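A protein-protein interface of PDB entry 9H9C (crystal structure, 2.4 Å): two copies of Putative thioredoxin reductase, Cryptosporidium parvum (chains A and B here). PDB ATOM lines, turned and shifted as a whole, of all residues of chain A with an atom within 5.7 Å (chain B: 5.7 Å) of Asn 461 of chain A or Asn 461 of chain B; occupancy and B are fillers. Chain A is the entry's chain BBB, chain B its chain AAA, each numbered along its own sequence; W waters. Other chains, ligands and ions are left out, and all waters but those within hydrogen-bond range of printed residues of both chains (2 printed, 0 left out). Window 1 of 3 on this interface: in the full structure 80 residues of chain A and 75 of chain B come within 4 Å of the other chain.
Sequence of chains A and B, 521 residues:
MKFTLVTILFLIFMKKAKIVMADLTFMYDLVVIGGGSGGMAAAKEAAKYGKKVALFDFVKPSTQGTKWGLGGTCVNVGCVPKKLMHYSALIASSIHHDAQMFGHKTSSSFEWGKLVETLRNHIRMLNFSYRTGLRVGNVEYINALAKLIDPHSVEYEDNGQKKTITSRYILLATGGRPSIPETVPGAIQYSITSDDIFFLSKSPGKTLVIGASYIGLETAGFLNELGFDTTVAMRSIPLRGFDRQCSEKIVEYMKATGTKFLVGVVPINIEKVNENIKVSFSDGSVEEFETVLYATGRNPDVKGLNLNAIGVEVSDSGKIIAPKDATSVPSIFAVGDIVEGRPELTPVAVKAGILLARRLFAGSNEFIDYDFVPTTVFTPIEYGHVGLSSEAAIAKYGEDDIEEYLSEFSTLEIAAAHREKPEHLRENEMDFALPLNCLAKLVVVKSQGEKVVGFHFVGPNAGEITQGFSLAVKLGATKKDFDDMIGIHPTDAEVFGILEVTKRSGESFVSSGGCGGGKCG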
ATOM      1  N   GLU A 382     -27.899 -17.467  10.431  1.00  0.00           N
ATOM      2  CA  GLU A 382     -27.162 -17.333   9.158  1.00  0.00           C
ATOM      3  C   GLU A 382     -27.799 -18.268   8.146  1.00  0.00           C
ATOM      4  O   GLU A 382     -28.476 -19.233   8.565  1.00  0.00           O
ATOM      5  CB  GLU A 382     -25.681 -17.674   9.366  1.00  0.00           C
ATOM      6  CG  GLU A 382     -25.097 -17.000  10.600  1.00  0.00           C
ATOM      7  CD  GLU A 382     -23.629 -17.226  10.852  1.00  0.00           C
ATOM      8  OE1 GLU A 382     -23.030 -18.218  10.285  1.00  0.00           O
ATOM      9  OE2 GLU A 382     -23.087 -16.399  11.585  1.00  0.00           O
ATOM     10  N   PHE A 457     -28.636 -24.389   4.378  1.00  0.00           N
ATOM     11  CA  PHE A 457     -28.577 -24.510   5.848  1.00  0.00           C
ATOM     12  C   PHE A 457     -28.775 -23.136   6.477  1.00  0.00           C
ATOM     13  O   PHE A 457     -27.995 -22.238   6.206  1.00  0.00           O
ATOM     14  CB  PHE A 457     -27.270 -25.130   6.332  1.00  0.00           C
ATOM     15  CG  PHE A 457     -27.256 -25.256   7.829  1.00  0.00           C
ATOM     16  CD1 PHE A 457     -27.932 -26.295   8.446  1.00  0.00           C
ATOM     17  CD2 PHE A 457     -26.652 -24.298   8.631  1.00  0.00           C
ATOM     18  CE1 PHE A 457     -27.978 -26.386   9.829  1.00  0.00           C
ATOM     19  CE2 PHE A 457     -26.697 -24.397  10.010  1.00  0.00           C
ATOM     20  CZ  PHE A 457     -27.358 -25.444  10.606  1.00  0.00           C
ATOM     21  N   GLY A 459     -29.058 -21.400  10.265  1.00  0.00           N
ATOM     22  CA  GLY A 459     -28.644 -21.695  11.649  1.00  0.00           C
ATOM     23  C   GLY A 459     -27.297 -21.057  12.003  1.00  0.00           C
ATOM     24  O   GLY A 459     -26.748 -20.291  11.222  1.00  0.00           O
ATOM     25  N   PRO A 460     -26.736 -21.342  13.189  1.00  0.00           N
ATOM     26  CA  PRO A 460     -25.427 -20.824  13.583  1.00  0.00           C
ATOM     27  C   PRO A 460     -24.299 -21.337  12.698  1.00  0.00           C
ATOM     28  O   PRO A 460     -24.405 -22.435  12.222  1.00  0.00           O
ATOM     29  CB  PRO A 460     -25.210 -21.311  15.019  1.00  0.00           C
ATOM     30  CG  PRO A 460     -26.585 -21.728  15.488  1.00  0.00           C
ATOM     31  CD  PRO A 460     -27.340 -22.167  14.244  1.00  0.00           C
ATOM     32  N   ASN A 461     -23.249 -20.538  12.507  1.00  0.00           N
ATOM     33  CA  ASN A 461     -22.036 -21.022  11.810  1.00  0.00           C
ATOM     34  C   ASN A 461     -22.433 -21.654  10.456  1.00  0.00           C
ATOM     35  O   ASN A 461     -21.880 -22.727  10.100  1.00  0.00           O
ATOM     36  CB  ASN A 461     -21.331 -22.028  12.704  1.00  0.00           C
ATOM     37  CG  ASN A 461     -21.262 -21.551  14.135  1.00  0.00           C
ATOM     38  OD1 ASN A 461     -20.740 -20.481  14.391  1.00  0.00           O
ATOM     39  ND2 ASN A 461     -21.804 -22.310  15.064  1.00  0.00           N
ATOM     40  N   ALA A 462     -23.311 -21.012   9.695  1.00  0.00           N
ATOM     41  CA  ALA A 462     -23.835 -21.623   8.456  1.00  0.00           C
ATOM     42  C   ALA A 462     -22.755 -21.641   7.379  1.00  0.00           C
ATOM     43  O   ALA A 462     -22.742 -22.554   6.563  1.00  0.00           O
ATOM     44  CB  ALA A 462     -25.092 -20.910   7.979  1.00  0.00           C
ATOM     45  N   GLY A 463     -21.945 -20.608   7.311  1.00  0.00           N
ATOM     46  CA  GLY A 463     -20.773 -20.565   6.408  1.00  0.00           C
ATOM     47  C   GLY A 463     -19.768 -21.657   6.746  1.00  0.00           C
ATOM     48  O   GLY A 463     -19.299 -22.354   5.842  1.00  0.00           O
ATOM     49  N   GLU A 464     -19.492 -21.850   8.023  1.00  0.00           N
ATOM     50  CA  GLU A 464     -18.531 -22.887   8.476  1.00  0.00           C
ATOM     51  C   GLU A 464     -19.094 -24.256   8.048  1.00  0.00           C
ATOM     52  O   GLU A 464     -18.314 -25.138   7.642  1.00  0.00           O
ATOM     53  CB  GLU A 464     -18.269 -22.755   9.978  1.00  0.00           C
ATOM     54  CG  GLU A 464     -17.803 -21.357  10.424  1.00  0.00           C
ATOM     55  CD  GLU A 464     -16.478 -20.808   9.924  1.00  0.00           C
ATOM     56  OE1 GLU A 464     -15.715 -21.559   9.305  1.00  0.00           O
ATOM     57  OE2 GLU A 464     -16.186 -19.596  10.222  1.00  0.00           O
ATOM     58  N   ILE A 465     -20.410 -24.437   8.083  1.00  0.00           N
ATOM     59  CA  ILE A 465     -21.049 -25.749   7.770  1.00  0.00           C
ATOM     60  C   ILE A 465     -21.064 -25.935   6.261  1.00  0.00           C
ATOM     61  O   ILE A 465     -20.843 -27.062   5.800  1.00  0.00           O
ATOM     62  CB  ILE A 465     -22.441 -25.854   8.414  1.00  0.00           C
ATOM     63  CG1 ILE A 465     -22.295 -26.001   9.931  1.00  0.00           C
ATOM     64  CG2 ILE A 465     -23.220 -27.007   7.821  1.00  0.00           C
ATOM     65  CD1 ILE A 465     -23.567 -25.789  10.729  1.00  0.00           C
ATOM     66  N   THR A 466     -21.261 -24.872   5.506  1.00  0.00           N
ATOM     67  CA  THR A 466     -21.584 -25.008   4.072  1.00  0.00           C
ATOM     68  C   THR A 466     -20.322 -25.204   3.252  1.00  0.00           C
ATOM     69  O   THR A 466     -20.425 -25.804   2.183  1.00  0.00           O
ATOM     70  CB  THR A 466     -22.353 -23.784   3.580  1.00  0.00           C
ATOM     71  OG1 THR A 466     -23.648 -23.790   4.190  1.00  0.00           O
ATOM     72  CG2 THR A 466     -22.500 -23.743   2.080  1.00  0.00           C
ATOM     73  N   GLU B 382     -11.222 -26.410  19.387  1.00  0.00           N
ATOM     74  CA  GLU B 382     -11.740 -27.749  19.055  1.00  0.00           C
ATOM     75  C   GLU B 382     -10.833 -28.372  18.006  1.00  0.00           C
ATOM     76  O   GLU B 382     -10.083 -27.630  17.349  1.00  0.00           O
ATOM     77  CB  GLU B 382     -13.161 -27.634  18.533  1.00  0.00           C
ATOM     78  CG  GLU B 382     -14.036 -26.775  19.425  1.00  0.00           C
ATOM     79  CD  GLU B 382     -15.492 -26.700  19.015  1.00  0.00           C
ATOM     80  OE1 GLU B 382     -15.818 -27.061  17.816  1.00  0.00           O
ATOM     81  OE2 GLU B 382     -16.309 -26.273  19.906  1.00  0.00           O
ATOM     82  N   PHE B 457      -8.539 -30.019  11.417  1.00  0.00           N
ATOM     83  CA  PHE B 457      -8.824 -28.589  11.661  1.00  0.00           C
ATOM     84  C   PHE B 457      -8.917 -28.359  13.151  1.00  0.00           C
ATOM     85  O   PHE B 457      -9.764 -28.995  13.800  1.00  0.00           O
ATOM     86  CB  PHE B 457     -10.100 -28.112  10.977  1.00  0.00           C
ATOM     87  CG  PHE B 457     -10.380 -26.663  11.272  1.00  0.00           C
ATOM     88  CD1 PHE B 457      -9.708 -25.676  10.571  1.00  0.00           C
ATOM     89  CD2 PHE B 457     -11.236 -26.284  12.296  1.00  0.00           C
ATOM     90  CE1 PHE B 457      -9.904 -24.342  10.874  1.00  0.00           C
ATOM     91  CE2 PHE B 457     -11.431 -24.945  12.583  1.00  0.00           C
ATOM     92  CZ  PHE B 457     -10.769 -23.980  11.878  1.00  0.00           C
ATOM     93  N   GLY B 459      -9.538 -25.281  15.843  1.00  0.00           N
ATOM     94  CA  GLY B 459     -10.139 -23.935  15.947  1.00  0.00           C
ATOM     95  C   GLY B 459     -11.616 -23.991  16.310  1.00  0.00           C
ATOM     96  O   GLY B 459     -12.120 -25.048  16.682  1.00  0.00           O
ATOM     97  N   PRO B 460     -12.347 -22.865  16.241  1.00  0.00           N
ATOM     98  CA  PRO B 460     -13.759 -22.838  16.600  1.00  0.00           C
ATOM     99  C   PRO B 460     -14.647 -23.684  15.692  1.00  0.00           C
ATOM    100  O   PRO B 460     -14.350 -23.791  14.586  1.00  0.00           O
ATOM    101  CB  PRO B 460     -14.178 -21.350  16.516  1.00  0.00           C
ATOM    102  CG  PRO B 460     -12.849 -20.613  16.546  1.00  0.00           C
ATOM    103  CD  PRO B 460     -11.861 -21.539  15.847  1.00  0.00           C
ATOM    104  N   ASN B 461     -15.725 -24.226  16.235  1.00  0.00           N
ATOM    105  CA  ASN B 461     -16.761 -24.919  15.430  1.00  0.00           C
ATOM    106  C   ASN B 461     -16.095 -25.982  14.528  1.00  0.00           C
ATOM    107  O   ASN B 461     -16.408 -26.056  13.295  1.00  0.00           O
ATOM    108  CB  ASN B 461     -17.522 -23.882  14.622  1.00  0.00           C
ATOM    109  CG  ASN B 461     -17.842 -22.649  15.439  1.00  0.00           C
ATOM    110  OD1 ASN B 461     -18.483 -22.757  16.510  1.00  0.00           O
ATOM    111  ND2 ASN B 461     -17.362 -21.503  14.952  1.00  0.00           N
ATOM    112  N   ALA B 462     -15.177 -26.759  15.071  1.00  0.00           N
ATOM    113  CA  ALA B 462     -14.348 -27.660  14.243  1.00  0.00           C
ATOM    114  C   ALA B 462     -15.202 -28.825  13.737  1.00  0.00           C
ATOM    115  O   ALA B 462     -14.936 -29.320  12.647  1.00  0.00           O
ATOM    116  CB  ALA B 462     -13.139 -28.139  15.013  1.00  0.00           C
ATOM    117  N   GLY B 463     -16.127 -29.313  14.537  1.00  0.00           N
ATOM    118  CA  GLY B 463     -17.093 -30.346  14.103  1.00  0.00           C
ATOM    119  C   GLY B 463     -17.995 -29.824  12.988  1.00  0.00           C
ATOM    120  O   GLY B 463     -18.189 -30.518  12.005  1.00  0.00           O
ATOM    121  N   GLU B 464     -18.495 -28.597  13.120  1.00  0.00           N
ATOM    122  CA  GLU B 464     -19.331 -27.959  12.078  1.00  0.00           C
ATOM    123  C   GLU B 464     -18.514 -27.892  10.779  1.00  0.00           C
ATOM    124  O   GLU B 464     -19.096 -28.127   9.694  1.00  0.00           O
ATOM    125  CB  GLU B 464     -19.847 -26.581  12.544  1.00  0.00           C
ATOM    126  CG  GLU B 464     -20.637 -26.586  13.871  1.00  0.00           C
ATOM    127  CD  GLU B 464     -21.958 -27.363  13.937  1.00  0.00           C
ATOM    128  OE1 GLU B 464     -22.423 -27.863  12.895  1.00  0.00           O
ATOM    129  OE2 GLU B 464     -22.593 -27.402  15.023  1.00  0.00           O
ATOM    130  N   ILE B 465     -17.214 -27.639  10.852  1.00  0.00           N
ATOM    131  CA  ILE B 465     -16.352 -27.447   9.657  1.00  0.00           C
ATOM    132  C   ILE B 465     -16.042 -28.817   9.058  1.00  0.00           C
ATOM    133  O   ILE B 465     -16.057 -28.962   7.815  1.00  0.00           O
ATOM    134  CB  ILE B 465     -15.088 -26.640  10.006  1.00  0.00           C
ATOM    135  CG1 ILE B 465     -15.472 -25.173  10.244  1.00  0.00           C
ATOM    136  CG2 ILE B 465     -14.076 -26.749   8.885  1.00  0.00           C
ATOM    137  CD1 ILE B 465     -14.414 -24.323  10.874  1.00  0.00           C
ATOM    138  N   THR B 466     -15.879 -29.835   9.894  1.00  0.00           N
ATOM    139  CA  THR B 466     -15.282 -31.099   9.443  1.00  0.00           C
ATOM    140  C   THR B 466     -16.328 -31.969   8.786  1.00  0.00           C
ATOM    141  O   THR B 466     -15.943 -32.799   7.953  1.00  0.00           O
ATOM    142  CB  THR B 466     -14.629 -31.850  10.608  1.00  0.00           C
ATOM    143  OG1 THR B 466     -13.500 -31.080  11.010  1.00  0.00           O
ATOM    144  CG2 THR B 466     -14.214 -33.252  10.238  1.00  0.00           C
HETATM  145  O   HOH W   1     -19.578 -29.145   7.226  1.00  0.00           O
HETATM  146  O   HOH W   2     -17.144 -27.190   6.291  1.00  0.00           O
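The side-chain carboxylate (OE1) of Glu 382 of chain B sits at hydrogen-bond distance from the backbone NH (N) of Asn 461 of chain B, 3.2 Å away. N of Asn 461 of chain A sits at hydrogen-bond distance from OE1 of Glu 382 of chain A (3.2 Å).
Among the printed residues, merely in contact across the chains: Ile 465 of chain A with Glu 464 of chain B (3.2 Å), Glu 464 of chain A with Ile 465 of chain B (3.4 Å), Asn 461 of chain A with Asn 461 of chain B (3.6 Å) and Glu 464 of chain A with Glu 464 of chain B (3.7 Å).
Water W2 lies within hydrogen-bond range of O of Ile 465 of chain B (2.6 Å) and O of Glu 464 of chain A (2.7 Å). Water W1 bridges the backbone carbonyl oxygen (O) of Glu 464 of chain B (2.7 Å) and the backbone carbonyl oxygen (O) of Ile 465 of chain A (2.8 Å).
Asn 461 of chain B touches its own counterpart, Asn 461 of chain A. Glu 464 of chain A touches its own counterpart, Glu 464 of chain B. Glu 464 of chain A touches Ile 465 of chain B, and with the chains exchanged Ile 465 of chain A touches Glu 464 of chain B. Positions printed for both chains: 382, 457, 459, 460, 461, 462, 463, 464, 465 and 466.
Asn 461 of chain A touches just one residue of chain B: Asn 461. Asn 461 of chain B touches just one residue of chain A: Asn 461 (3.6 Å). Printed residues of chain B within 4 Å of Ile 465 of chain A: Glu 464 (3.2 Å). Of the printed residues of chain B, Glu 464 of chain A touches Glu 464 and Ile 465. Printed residues of chain A within 4 Å of Ile 465 of chain B: Glu 464 (3.4 Å). Phe 457 of chain B touches none of the printed residues of chain A. Glu 382 of chain B touches none of the printed residues of chain A. The nearest residue of chain B that does not touch Asn 461 of chain A is Glu 464 of chain B (4.6 Å). The nearest residue of chain A that does not touch Asn 461 of chain B is Glu 464 of chain A (4.6 Å).
Hydrophobic or aromatic side chains of chain B within 4 Å of the printed part of chain A: Ile 465. Printed residues of chain A that touch a printed residue of chain B: Asn 461, Glu 464 and Ile 465.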
